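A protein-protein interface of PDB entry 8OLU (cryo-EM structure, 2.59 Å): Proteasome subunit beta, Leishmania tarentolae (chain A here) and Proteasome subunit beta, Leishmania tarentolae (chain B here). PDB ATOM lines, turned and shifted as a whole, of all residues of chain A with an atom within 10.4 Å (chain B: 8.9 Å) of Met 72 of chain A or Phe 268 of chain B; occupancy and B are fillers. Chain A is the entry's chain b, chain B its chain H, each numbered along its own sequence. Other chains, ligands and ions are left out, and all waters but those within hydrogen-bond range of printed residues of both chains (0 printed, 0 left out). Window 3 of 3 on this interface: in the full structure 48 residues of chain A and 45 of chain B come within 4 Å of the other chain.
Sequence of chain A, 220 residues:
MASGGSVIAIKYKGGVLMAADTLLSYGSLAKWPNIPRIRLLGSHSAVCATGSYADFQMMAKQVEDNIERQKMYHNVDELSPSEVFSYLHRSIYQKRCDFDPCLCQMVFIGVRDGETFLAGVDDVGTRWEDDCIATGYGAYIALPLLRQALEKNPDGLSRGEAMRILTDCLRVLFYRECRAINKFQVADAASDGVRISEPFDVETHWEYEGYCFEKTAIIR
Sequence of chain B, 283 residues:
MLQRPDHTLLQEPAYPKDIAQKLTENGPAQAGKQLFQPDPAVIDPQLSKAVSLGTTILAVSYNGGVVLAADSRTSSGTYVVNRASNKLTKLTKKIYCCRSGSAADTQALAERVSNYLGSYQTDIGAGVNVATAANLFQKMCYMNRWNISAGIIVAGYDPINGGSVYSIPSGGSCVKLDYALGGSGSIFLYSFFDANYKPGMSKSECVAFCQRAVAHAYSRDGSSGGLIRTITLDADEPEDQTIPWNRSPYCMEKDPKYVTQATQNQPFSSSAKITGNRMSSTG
Of the printed residues of chain B, Arg 39 of chain A touches Asn 265. Asp 65 of chain A touches none of the printed residues of chain B. Met 72 of chain A touches just one residue of chain B: Phe 268. Of the printed residues of chain A, Asn 265 of chain B touches Arg 39. No residue of chain A comes within 4 Å of Pro 267 of chain B. Ser 269 of chain B touches none of the printed residues of chain A. Thr 275 of chain B touches none of the printed residues of chain A. The nearest printed residue of chain A that does not touch Asn 265 of chain B is Leu 40 of chain A (5.7 Å).
Among the printed residues, merely in contact across the chains: Leu 40 of chain A with Arg 278 of chain B (3.7 Å), Glu 68 of chain A with Phe 268 of chain B (3.5 Å) and Met 72 of chain A with Phe 268 of chain B (3.5 Å).
The guanidinium group (NH1) of Arg 278 of chain B is in hydrogen-bond range of the backbone carbonyl oxygen (O) of Gly 42 of chain A. NE of Arg 39 of chain A is in hydrogen-bond range of OD1 of Asn 265 of chain B, 3.0 Å away.
Of the 13 printed residues of chain B, 3 touch a printed residue of chain A. Printed residues of chain B that touch a printed residue of chain A: Asn 265, Phe 268 and Arg 278. Of the 23 printed residues of chain A, 5 touch a printed residue of chain B. Hydrophobic or aromatic side chains of chain A within 4 Å of the printed part of chain B: Leu 40 and Met 72. Among the printed residues, no Asp or Glu carboxylate lies within 4 Å of a Lys or Arg side-chain nitrogen of the other chain.
The guanidinium group of Arg 39 of chain A is in salt-bridge range of the side-chain carboxylate of Glu 64 of chain A (3.5 Å). O of Asn 265 of chain B is in hydrogen-bond range of N of Arg 278 of chain B. N of Asn 265 of chain B is in hydrogen-bond range of OD1 of Asn 277 of chain B, at 2.8 Å.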
ATOM      1  N   ARG A  39      38.455  -1.939  37.696  1.00  0.00           N
ATOM      2  CA  ARG A  39      37.769  -2.726  36.709  1.00  0.00           C
ATOM      3  C   ARG A  39      36.666  -1.912  36.065  1.00  0.00           C
ATOM      4  O   ARG A  39      35.869  -1.349  36.760  1.00  0.00           O
ATOM      5  CB  ARG A  39      37.253  -3.961  37.421  1.00  0.00           C
ATOM      6  CG  ARG A  39      35.990  -4.514  36.829  1.00  0.00           C
ATOM      7  CD  ARG A  39      36.351  -5.780  36.163  1.00  0.00           C
ATOM      8  NE  ARG A  39      36.661  -6.684  37.256  1.00  0.00           N
ATOM      9  CZ  ARG A  39      36.376  -7.973  37.228  1.00  0.00           C
ATOM     10  NH1 ARG A  39      35.450  -8.415  36.396  1.00  0.00           N
ATOM     11  NH2 ARG A  39      37.032  -8.786  38.038  1.00  0.00           N
ATOM     12  N   LEU A  40      36.641  -1.878  34.745  1.00  0.00           N
ATOM     13  CA  LEU A  40      35.583  -1.251  34.015  1.00  0.00           C
ATOM     14  C   LEU A  40      34.320  -2.074  34.067  1.00  0.00           C
ATOM     15  O   LEU A  40      34.356  -3.302  34.053  1.00  0.00           O
ATOM     16  CB  LEU A  40      36.042  -1.137  32.594  1.00  0.00           C
ATOM     17  CG  LEU A  40      37.321  -0.335  32.417  1.00  0.00           C
ATOM     18  CD1 LEU A  40      37.503   0.001  30.986  1.00  0.00           C
ATOM     19  CD2 LEU A  40      37.340   0.994  33.166  1.00  0.00           C
ATOM     20  N   LEU A  41      33.194  -1.368  34.124  1.00  0.00           N
ATOM     21  CA  LEU A  41      31.882  -1.935  34.227  1.00  0.00           C
ATOM     22  C   LEU A  41      31.057  -1.268  33.173  1.00  0.00           C
ATOM     23  O   LEU A  41      30.618  -0.118  33.320  1.00  0.00           O
ATOM     24  CB  LEU A  41      31.234  -1.556  35.551  1.00  0.00           C
ATOM     25  CG  LEU A  41      31.864  -2.129  36.806  1.00  0.00           C
ATOM     26  CD1 LEU A  41      31.125  -1.592  38.011  1.00  0.00           C
ATOM     27  CD2 LEU A  41      31.823  -3.646  36.827  1.00  0.00           C
ATOM     28  N   GLY A  42      30.806  -1.981  32.113  1.00  0.00           N
ATOM     29  CA  GLY A  42      29.964  -1.394  31.093  1.00  0.00           C
ATOM     30  C   GLY A  42      30.807  -0.420  30.339  1.00  0.00           C
ATOM     31  O   GLY A  42      32.013  -0.499  30.439  1.00  0.00           O
ATOM     32  N   SER A  43      30.144   0.524  29.713  1.00  0.00           N
ATOM     33  CA  SER A  43      30.800   1.469  28.838  1.00  0.00           C
ATOM     34  C   SER A  43      31.126   2.777  29.513  1.00  0.00           C
ATOM     35  O   SER A  43      31.793   3.575  28.888  1.00  0.00           O
ATOM     36  CB  SER A  43      29.923   1.718  27.688  1.00  0.00           C
ATOM     37  OG  SER A  43      29.609   0.466  27.057  1.00  0.00           O
ATOM     38  N   LYS A  61      31.708  -9.348  39.049  1.00  0.00           N
ATOM     39  CA  LYS A  61      31.259 -10.168  37.961  1.00  0.00           C
ATOM     40  C   LYS A  61      29.733 -10.100  37.841  1.00  0.00           C
ATOM     41  O   LYS A  61      29.207  -9.972  36.765  1.00  0.00           O
ATOM     42  CB  LYS A  61      31.737 -11.589  38.222  1.00  0.00           C
ATOM     43  CG  LYS A  61      31.582 -12.518  37.049  1.00  0.00           C
ATOM     44  CD  LYS A  61      31.301 -13.881  37.566  1.00  0.00           C
ATOM     45  CE  LYS A  61      30.974 -14.849  36.443  1.00  0.00           C
ATOM     46  NZ  LYS A  61      31.363 -16.233  36.840  1.00  0.00           N
ATOM     47  N   VAL A  63      27.807  -7.713  38.628  1.00  0.00           N
ATOM     48  CA  VAL A  63      27.354  -6.448  38.100  1.00  0.00           C
ATOM     49  C   VAL A  63      27.669  -6.343  36.636  1.00  0.00           C
ATOM     50  O   VAL A  63      26.870  -5.802  35.954  1.00  0.00           O
ATOM     51  CB  VAL A  63      28.004  -5.276  38.847  1.00  0.00           C
ATOM     52  CG1 VAL A  63      27.778  -3.917  38.174  1.00  0.00           C
ATOM     53  CG2 VAL A  63      27.574  -5.209  40.306  1.00  0.00           C
ATOM     54  N   GLU A  64      28.876  -6.696  36.203  1.00  0.00           N
ATOM     55  CA  GLU A  64      29.258  -6.654  34.808  1.00  0.00           C
ATOM     56  C   GLU A  64      28.234  -7.424  33.993  1.00  0.00           C
ATOM     57  O   GLU A  64      27.830  -6.975  32.930  1.00  0.00           O
ATOM     58  CB  GLU A  64      30.580  -7.358  34.531  1.00  0.00           C
ATOM     59  CG  GLU A  64      31.770  -6.464  34.196  1.00  0.00           C
ATOM     60  CD  GLU A  64      33.166  -7.107  34.367  1.00  0.00           C
ATOM     61  OE1 GLU A  64      33.652  -7.254  35.541  1.00  0.00           O
ATOM     62  OE2 GLU A  64      33.797  -7.462  33.327  1.00  0.00           O
ATOM     63  N   ASP A  65      27.873  -8.608  34.480  1.00  0.00           N
ATOM     64  CA  ASP A  65      26.991  -9.504  33.765  1.00  0.00           C
ATOM     65  C   ASP A  65      25.602  -8.915  33.655  1.00  0.00           C
ATOM     66  O   ASP A  65      25.024  -8.884  32.583  1.00  0.00           O
ATOM     67  CB  ASP A  65      26.864 -10.853  34.457  1.00  0.00           C
ATOM     68  CG  ASP A  65      28.144 -11.687  34.341  1.00  0.00           C
ATOM     69  OD1 ASP A  65      29.160 -11.184  33.688  1.00  0.00           O
ATOM     70  OD2 ASP A  65      28.167 -12.835  34.945  1.00  0.00           O
ATOM     71  N   ASN A  66      25.093  -8.433  34.762  1.00  0.00           N
ATOM     72  CA  ASN A  66      23.819  -7.783  34.785  1.00  0.00           C
ATOM     73  C   ASN A  66      23.787  -6.675  33.761  1.00  0.00           C
ATOM     74  O   ASN A  66      22.875  -6.563  32.988  1.00  0.00           O
ATOM     75  CB  ASN A  66      23.586  -7.283  36.188  1.00  0.00           C
ATOM     76  CG  ASN A  66      22.239  -6.644  36.361  1.00  0.00           C
ATOM     77  OD1 ASN A  66      22.139  -5.434  36.515  1.00  0.00           O
ATOM     78  ND2 ASN A  66      21.209  -7.449  36.258  1.00  0.00           N
ATOM     79  N   ILE A  67      24.817  -5.889  33.689  1.00  0.00           N
ATOM     80  CA  ILE A  67      24.838  -4.809  32.734  1.00  0.00           C
ATOM     81  C   ILE A  67      24.782  -5.312  31.308  1.00  0.00           C
ATOM     82  O   ILE A  67      24.140  -4.720  30.465  1.00  0.00           O
ATOM     83  CB  ILE A  67      26.108  -3.975  32.915  1.00  0.00           C
ATOM     84  CG1 ILE A  67      26.107  -3.286  34.254  1.00  0.00           C
ATOM     85  CG2 ILE A  67      26.291  -2.931  31.836  1.00  0.00           C
ATOM     86  CD1 ILE A  67      27.430  -2.597  34.505  1.00  0.00           C
ATOM     87  N   GLU A  68      25.603  -6.292  31.025  1.00  0.00           N
ATOM     88  CA  GLU A  68      25.814  -6.750  29.683  1.00  0.00           C
ATOM     89  C   GLU A  68      24.556  -7.460  29.164  1.00  0.00           C
ATOM     90  O   GLU A  68      24.164  -7.290  28.016  1.00  0.00           O
ATOM     91  CB  GLU A  68      27.069  -7.627  29.722  1.00  0.00           C
ATOM     92  CG  GLU A  68      27.698  -7.777  28.353  1.00  0.00           C
ATOM     93  CD  GLU A  68      27.551  -6.595  27.369  1.00  0.00           C
ATOM     94  OE1 GLU A  68      28.454  -5.669  27.407  1.00  0.00           O
ATOM     95  OE2 GLU A  68      26.523  -6.593  26.542  1.00  0.00           O
ATOM     96  N   ARG A  69      23.946  -8.258  30.029  1.00  0.00           N
ATOM     97  CA  ARG A  69      22.775  -9.003  29.685  1.00  0.00           C
ATOM     98  C   ARG A  69      21.570  -8.103  29.548  1.00  0.00           C
ATOM     99  O   ARG A  69      20.757  -8.282  28.677  1.00  0.00           O
ATOM    100  CB  ARG A  69      22.512 -10.018  30.782  1.00  0.00           C
ATOM    101  CG  ARG A  69      23.577 -11.103  30.779  1.00  0.00           C
ATOM    102  CD  ARG A  69      23.538 -12.054  31.952  1.00  0.00           C
ATOM    103  NE  ARG A  69      24.824 -12.758  31.906  1.00  0.00           N
ATOM    104  CZ  ARG A  69      25.224 -13.644  32.829  1.00  0.00           C
ATOM    105  NH1 ARG A  69      24.487 -13.879  33.915  1.00  0.00           N
ATOM    106  NH2 ARG A  69      26.333 -14.327  32.591  1.00  0.00           N
ATOM    107  N   GLN A  70      21.401  -7.130  30.416  1.00  0.00           N
ATOM    108  CA  GLN A  70      20.261  -6.251  30.311  1.00  0.00           C
ATOM    109  C   GLN A  70      20.286  -5.674  28.912  1.00  0.00           C
ATOM    110  O   GLN A  70      19.267  -5.560  28.295  1.00  0.00           O
ATOM    111  CB  GLN A  70      20.303  -5.197  31.415  1.00  0.00           C
ATOM    112  CG  GLN A  70      18.939  -4.656  31.797  1.00  0.00           C
ATOM    113  CD  GLN A  70      18.754  -3.155  31.632  1.00  0.00           C
ATOM    114  OE1 GLN A  70      19.572  -2.463  31.005  1.00  0.00           O
ATOM    115  NE2 GLN A  70      17.641  -2.650  32.167  1.00  0.00           N
ATOM    116  N   LYS A  71      21.448  -5.419  28.375  1.00  0.00           N
ATOM    117  CA  LYS A  71      21.587  -4.639  27.177  1.00  0.00           C
ATOM    118  C   LYS A  71      21.556  -5.493  25.917  1.00  0.00           C
ATOM    119  O   LYS A  71      21.245  -5.020  24.827  1.00  0.00           O
ATOM    120  CB  LYS A  71      22.986  -4.063  27.287  1.00  0.00           C
ATOM    121  CG  LYS A  71      23.444  -3.153  26.174  1.00  0.00           C
ATOM    122  CD  LYS A  71      24.945  -2.878  26.199  1.00  0.00           C
ATOM    123  CE  LYS A  71      25.190  -1.680  25.291  1.00  0.00           C
ATOM    124  NZ  LYS A  71      26.368  -1.841  24.405  1.00  0.00           N
ATOM    125  N   MET A  72      22.023  -6.727  26.042  1.00  0.00           N
ATOM    126  CA  MET A  72      22.151  -7.634  24.924  1.00  0.00           C
ATOM    127  C   MET A  72      20.796  -8.265  24.704  1.00  0.00           C
ATOM    128  O   MET A  72      20.368  -8.404  23.564  1.00  0.00           O
ATOM    129  CB  MET A  72      23.201  -8.677  25.274  1.00  0.00           C
ATOM    130  CG  MET A  72      23.199 -10.037  24.586  1.00  0.00           C
ATOM    131  SD  MET A  72      24.564 -11.067  25.444  1.00  0.00           S
ATOM    132  CE  MET A  72      25.927 -10.185  24.700  1.00  0.00           C
ATOM    133  N   TYR A  73      20.110  -8.530  25.801  1.00  0.00           N
ATOM    134  CA  TYR A  73      18.834  -9.185  25.733  1.00  0.00           C
ATOM    135  C   TYR A  73      17.641  -8.297  25.468  1.00  0.00           C
ATOM    136  O   TYR A  73      16.596  -8.831  25.179  1.00  0.00           O
ATOM    137  CB  TYR A  73      18.436  -9.786  27.067  1.00  0.00           C
ATOM    138  CG  TYR A  73      19.326 -10.883  27.575  1.00  0.00           C
ATOM    139  CD1 TYR A  73      20.365 -11.401  26.804  1.00  0.00           C
ATOM    140  CD2 TYR A  73      19.097 -11.405  28.837  1.00  0.00           C
ATOM    141  CE1 TYR A  73      21.220 -12.368  27.323  1.00  0.00           C
ATOM    142  CE2 TYR A  73      19.924 -12.394  29.352  1.00  0.00           C
ATOM    143  CZ  TYR A  73      20.994 -12.856  28.602  1.00  0.00           C
ATOM    144  OH  TYR A  73      21.777 -13.835  29.147  1.00  0.00           O
ATOM    145  N   HIS A  74      17.697  -7.021  25.779  1.00  0.00           N
ATOM    146  CA  HIS A  74      16.597  -6.126  25.487  1.00  0.00           C
ATOM    147  C   HIS A  74      17.127  -4.981  24.642  1.00  0.00           C
ATOM    148  O   HIS A  74      18.296  -4.640  24.655  1.00  0.00           O
ATOM    149  CB  HIS A  74      15.976  -5.658  26.778  1.00  0.00           C
ATOM    150  CG  HIS A  74      15.636  -6.744  27.746  1.00  0.00           C
ATOM    151  ND1 HIS A  74      14.680  -7.696  27.522  1.00  0.00           N
ATOM    152  CD2 HIS A  74      16.160  -6.978  28.989  1.00  0.00           C
ATOM    153  CE1 HIS A  74      14.641  -8.507  28.594  1.00  0.00           C
ATOM    154  NE2 HIS A  74      15.562  -8.089  29.519  1.00  0.00           N
ATOM    155  N   ASN A  75      16.304  -4.435  23.788  1.00  0.00           N
ATOM    156  CA  ASN A  75      16.839  -3.400  22.929  1.00  0.00           C
ATOM    157  C   ASN A  75      16.832  -2.120  23.759  1.00  0.00           C
ATOM    158  O   ASN A  75      16.101  -1.193  23.411  1.00  0.00           O
ATOM    159  CB  ASN A  75      16.071  -3.298  21.590  1.00  0.00           C
ATOM    160  CG  ASN A  75      16.221  -1.968  20.849  1.00  0.00           C
ATOM    161  OD1 ASN A  75      15.271  -1.496  20.216  1.00  0.00           O
ATOM    162  ND2 ASN A  75      17.414  -1.382  20.869  1.00  0.00           N
ATOM    163  N   VAL A  76      17.629  -2.065  24.834  1.00  0.00           N
ATOM    164  CA  VAL A  76      17.562  -0.934  25.756  1.00  0.00           C
ATOM    165  C   VAL A  76      18.914  -0.271  25.834  1.00  0.00           C
ATOM    166  O   VAL A  76      19.914  -0.845  25.440  1.00  0.00           O
ATOM    167  CB  VAL A  76      17.125  -1.329  27.167  1.00  0.00           C
ATOM    168  CG1 VAL A  76      15.708  -1.861  27.216  1.00  0.00           C
ATOM    169  CG2 VAL A  76      18.086  -2.328  27.786  1.00  0.00           C
ATOM    170  N   ASP A  77      18.913   0.955  26.332  1.00  0.00           N
ATOM    171  CA  ASP A  77      20.153   1.692  26.536  1.00  0.00           C
ATOM    172  C   ASP A  77      20.857   1.068  27.727  1.00  0.00           C
ATOM    173  O   ASP A  77      20.223   0.759  28.720  1.00  0.00           O
ATOM    174  CB  ASP A  77      19.905   3.183  26.806  1.00  0.00           C
ATOM    175  CG  ASP A  77      19.340   3.966  25.618  1.00  0.00           C
ATOM    176  OD1 ASP A  77      19.682   5.161  25.476  1.00  0.00           O
ATOM    177  OD2 ASP A  77      18.572   3.373  24.821  1.00  0.00           O
ATOM    178  N   GLU A  78      22.157   0.892  27.613  1.00  0.00           N
ATOM    179  CA  GLU A  78      22.967   0.549  28.759  1.00  0.00           C
ATOM    180  C   GLU A  78      22.584   1.356  30.002  1.00  0.00           C
ATOM    181  O   GLU A  78      22.158   2.492  29.945  1.00  0.00           O
ATOM    182  CB  GLU A  78      24.422   0.855  28.428  1.00  0.00           C
ATOM    183  CG  GLU A  78      25.398   0.081  29.277  1.00  0.00           C
ATOM    184  CD  GLU A  78      26.863   0.195  28.887  1.00  0.00           C
ATOM    185  OE1 GLU A  78      27.201   0.018  27.667  1.00  0.00           O
ATOM    186  OE2 GLU A  78      27.672   0.413  29.813  1.00  0.00           O
ATOM    187  N   LEU A  79      22.765   0.724  31.128  1.00  0.00           N
ATOM    188  CA  LEU A  79      22.469   1.318  32.381  1.00  0.00           C
ATOM    189  C   LEU A  79      23.399   2.479  32.593  1.00  0.00           C
ATOM    190  O   LEU A  79      24.599   2.403  32.319  1.00  0.00           O
ATOM    191  CB  LEU A  79      22.806   0.312  33.469  1.00  0.00           C
ATOM    192  CG  LEU A  79      21.809  -0.824  33.643  1.00  0.00           C
ATOM    193  CD1 LEU A  79      22.392  -1.860  34.574  1.00  0.00           C
ATOM    194  CD2 LEU A  79      20.459  -0.320  34.164  1.00  0.00           C
ATOM    195  N   ASN B 265      40.886  -8.877  34.290  1.00  0.00           N
ATOM    196  CA  ASN B 265      39.750  -8.088  33.933  1.00  0.00           C
ATOM    197  C   ASN B 265      39.611  -8.217  32.430  1.00  0.00           C
ATOM    198  O   ASN B 265      39.787  -7.243  31.699  1.00  0.00           O
ATOM    199  CB  ASN B 265      39.994  -6.627  34.258  1.00  0.00           C
ATOM    200  CG  ASN B 265      40.182  -6.355  35.726  1.00  0.00           C
ATOM    201  OD1 ASN B 265      39.585  -7.027  36.569  1.00  0.00           O
ATOM    202  ND2 ASN B 265      40.953  -5.311  36.000  1.00  0.00           N
ATOM    203  N   GLN B 266      39.380  -9.444  31.991  1.00  0.00           N
ATOM    204  CA  GLN B 266      39.309  -9.731  30.585  1.00  0.00           C
ATOM    205  C   GLN B 266      38.129  -8.997  30.014  1.00  0.00           C
ATOM    206  O   GLN B 266      37.120  -8.862  30.668  1.00  0.00           O
ATOM    207  CB  GLN B 266      39.077 -11.211  30.384  1.00  0.00           C
ATOM    208  CG  GLN B 266      40.312 -12.086  30.510  1.00  0.00           C
ATOM    209  CD  GLN B 266      39.811 -13.512  30.464  1.00  0.00           C
ATOM    210  OE1 GLN B 266      39.099 -13.910  29.536  1.00  0.00           O
ATOM    211  NE2 GLN B 266      40.085 -14.262  31.513  1.00  0.00           N
ATOM    212  N   PRO B 267      38.190  -8.524  28.778  1.00  0.00           N
ATOM    213  CA  PRO B 267      36.994  -8.033  28.119  1.00  0.00           C
ATOM    214  C   PRO B 267      36.124  -9.192  27.726  1.00  0.00           C
ATOM    215  O   PRO B 267      36.648 -10.242  27.339  1.00  0.00           O
ATOM    216  CB  PRO B 267      37.398  -7.475  26.765  1.00  0.00           C
ATOM    217  CG  PRO B 267      38.822  -7.888  26.597  1.00  0.00           C
ATOM    218  CD  PRO B 267      39.349  -8.484  27.915  1.00  0.00           C
ATOM    219  N   PHE B 268      34.826  -8.887  27.693  1.00  0.00           N
ATOM    220  CA  PHE B 268      33.761  -9.755  27.205  1.00  0.00           C
ATOM    221  C   PHE B 268      34.050 -10.181  25.782  1.00  0.00           C
ATOM    222  O   PHE B 268      34.222  -9.327  24.908  1.00  0.00           O
ATOM    223  CB  PHE B 268      32.475  -8.948  27.171  1.00  0.00           C
ATOM    224  CG  PHE B 268      31.230  -9.771  27.111  1.00  0.00           C
ATOM    225  CD1 PHE B 268      31.058 -10.844  27.964  1.00  0.00           C
ATOM    226  CD2 PHE B 268      30.211  -9.413  26.256  1.00  0.00           C
ATOM    227  CE1 PHE B 268      29.904 -11.606  27.899  1.00  0.00           C
ATOM    228  CE2 PHE B 268      29.058 -10.161  26.224  1.00  0.00           C
ATOM    229  CZ  PHE B 268      28.917 -11.270  27.027  1.00  0.00           C
ATOM    230  N   SER B 269      34.219 -11.492  25.575  1.00  0.00           N
ATOM    231  CA  SER B 269      34.568 -11.919  24.242  1.00  0.00           C
ATOM    232  C   SER B 269      33.778 -13.146  23.820  1.00  0.00           C
ATOM    233  O   SER B 269      33.190 -13.845  24.630  1.00  0.00           O
ATOM    234  CB  SER B 269      36.059 -12.087  24.113  1.00  0.00           C
ATOM    235  OG  SER B 269      36.477 -13.407  24.358  1.00  0.00           O
ATOM    236  N   SER B 270      33.846 -13.395  22.521  1.00  0.00           N
ATOM    237  CA  SER B 270      33.243 -14.551  21.912  1.00  0.00           C
ATOM    238  C   SER B 270      34.199 -15.737  22.003  1.00  0.00           C
ATOM    239  O   SER B 270      33.896 -16.833  21.541  1.00  0.00           O
ATOM    240  CB  SER B 270      32.925 -14.205  20.506  1.00  0.00           C
ATOM    241  OG  SER B 270      32.157 -12.991  20.448  1.00  0.00           O
ATOM    242  N   SER B 271      35.381 -15.538  22.579  1.00  0.00           N
ATOM    243  CA  SER B 271      36.317 -16.635  22.650  1.00  0.00           C
ATOM    244  C   SER B 271      36.811 -16.841  24.079  1.00  0.00           C
ATOM    245  O   SER B 271      36.621 -16.016  24.965  1.00  0.00           O
ATOM    246  CB  SER B 271      37.451 -16.447  21.677  1.00  0.00           C
ATOM    247  OG  SER B 271      38.464 -17.433  21.840  1.00  0.00           O
ATOM    248  N   ALA B 272      37.375 -18.027  24.295  1.00  0.00           N
ATOM    249  CA  ALA B 272      38.080 -18.342  25.510  1.00  0.00           C
ATOM    250  C   ALA B 272      39.534 -17.851  25.482  1.00  0.00           C
ATOM    251  O   ALA B 272      40.204 -17.880  26.525  1.00  0.00           O
ATOM    252  CB  ALA B 272      38.026 -19.822  25.712  1.00  0.00           C
ATOM    253  N   LYS B 273      40.029 -17.496  24.287  1.00  0.00           N
ATOM    254  CA  LYS B 273      41.382 -16.992  24.146  1.00  0.00           C
ATOM    255  C   LYS B 273      41.500 -15.711  24.966  1.00  0.00           C
ATOM    256  O   LYS B 273      40.751 -14.757  24.767  1.00  0.00           O
ATOM    257  CB  LYS B 273      41.698 -16.792  22.667  1.00  0.00           C
ATOM    258  CG  LYS B 273      42.991 -16.073  22.333  1.00  0.00           C
ATOM    259  CD  LYS B 273      44.189 -16.608  23.079  1.00  0.00           C
ATOM    260  CE  LYS B 273      45.485 -15.918  22.694  1.00  0.00           C
ATOM    261  NZ  LYS B 273      45.913 -16.396  21.357  1.00  0.00           N
ATOM    262  N   THR B 275      43.410 -12.409  26.209  1.00  0.00           N
ATOM    263  CA  THR B 275      44.082 -11.368  25.443  1.00  0.00           C
ATOM    264  C   THR B 275      44.885 -10.488  26.399  1.00  0.00           C
ATOM    265  O   THR B 275      46.043 -10.168  26.134  1.00  0.00           O
ATOM    266  CB  THR B 275      43.085 -10.583  24.551  1.00  0.00           C
ATOM    267  OG1 THR B 275      41.981 -10.022  25.275  1.00  0.00           O
ATOM    268  CG2 THR B 275      42.498 -11.467  23.458  1.00  0.00           C
ATOM    269  N   GLY B 276      44.294 -10.118  27.532  1.00  0.00           N
ATOM    270  CA  GLY B 276      44.695  -8.878  28.156  1.00  0.00           C
ATOM    271  C   GLY B 276      43.600  -8.316  29.042  1.00  0.00           C
ATOM    272  O   GLY B 276      42.524  -8.865  29.149  1.00  0.00           O
ATOM    273  N   ASN B 277      43.942  -7.285  29.783  1.00  0.00           N
ATOM    274  CA  ASN B 277      42.961  -6.671  30.624  1.00  0.00           C
ATOM    275  C   ASN B 277      42.253  -5.645  29.774  1.00  0.00           C
ATOM    276  O   ASN B 277      42.851  -5.104  28.864  1.00  0.00           O
ATOM    277  CB  ASN B 277      43.628  -6.050  31.830  1.00  0.00           C
ATOM    278  CG  ASN B 277      44.098  -7.080  32.808  1.00  0.00           C
ATOM    279  OD1 ASN B 277      43.274  -7.834  33.302  1.00  0.00           O
ATOM    280  ND2 ASN B 277      45.377  -7.074  33.136  1.00  0.00           N
ATOM    281  N   ARG B 278      40.999  -5.388  30.102  1.00  0.00           N
ATOM    282  CA  ARG B 278      40.267  -4.359  29.417  1.00  0.00           C
ATOM    283  C   ARG B 278      40.698  -3.022  29.999  1.00  0.00           C
ATOM    284  O   ARG B 278      40.367  -2.705  31.125  1.00  0.00           O
ATOM    285  CB  ARG B 278      38.775  -4.681  29.544  1.00  0.00           C
ATOM    286  CG  ARG B 278      37.846  -3.637  28.941  1.00  0.00           C
ATOM    287  CD  ARG B 278      36.415  -3.984  29.288  1.00  0.00           C
ATOM    288  NE  ARG B 278      35.598  -3.042  28.525  1.00  0.00           N
ATOM    289  CZ  ARG B 278      34.512  -2.437  28.979  1.00  0.00           C
ATOM    290  NH1 ARG B 278      33.979  -1.432  28.305  1.00  0.00           N
ATOM    291  NH2 ARG B 278      33.978  -2.859  30.108  1.00  0.00           N
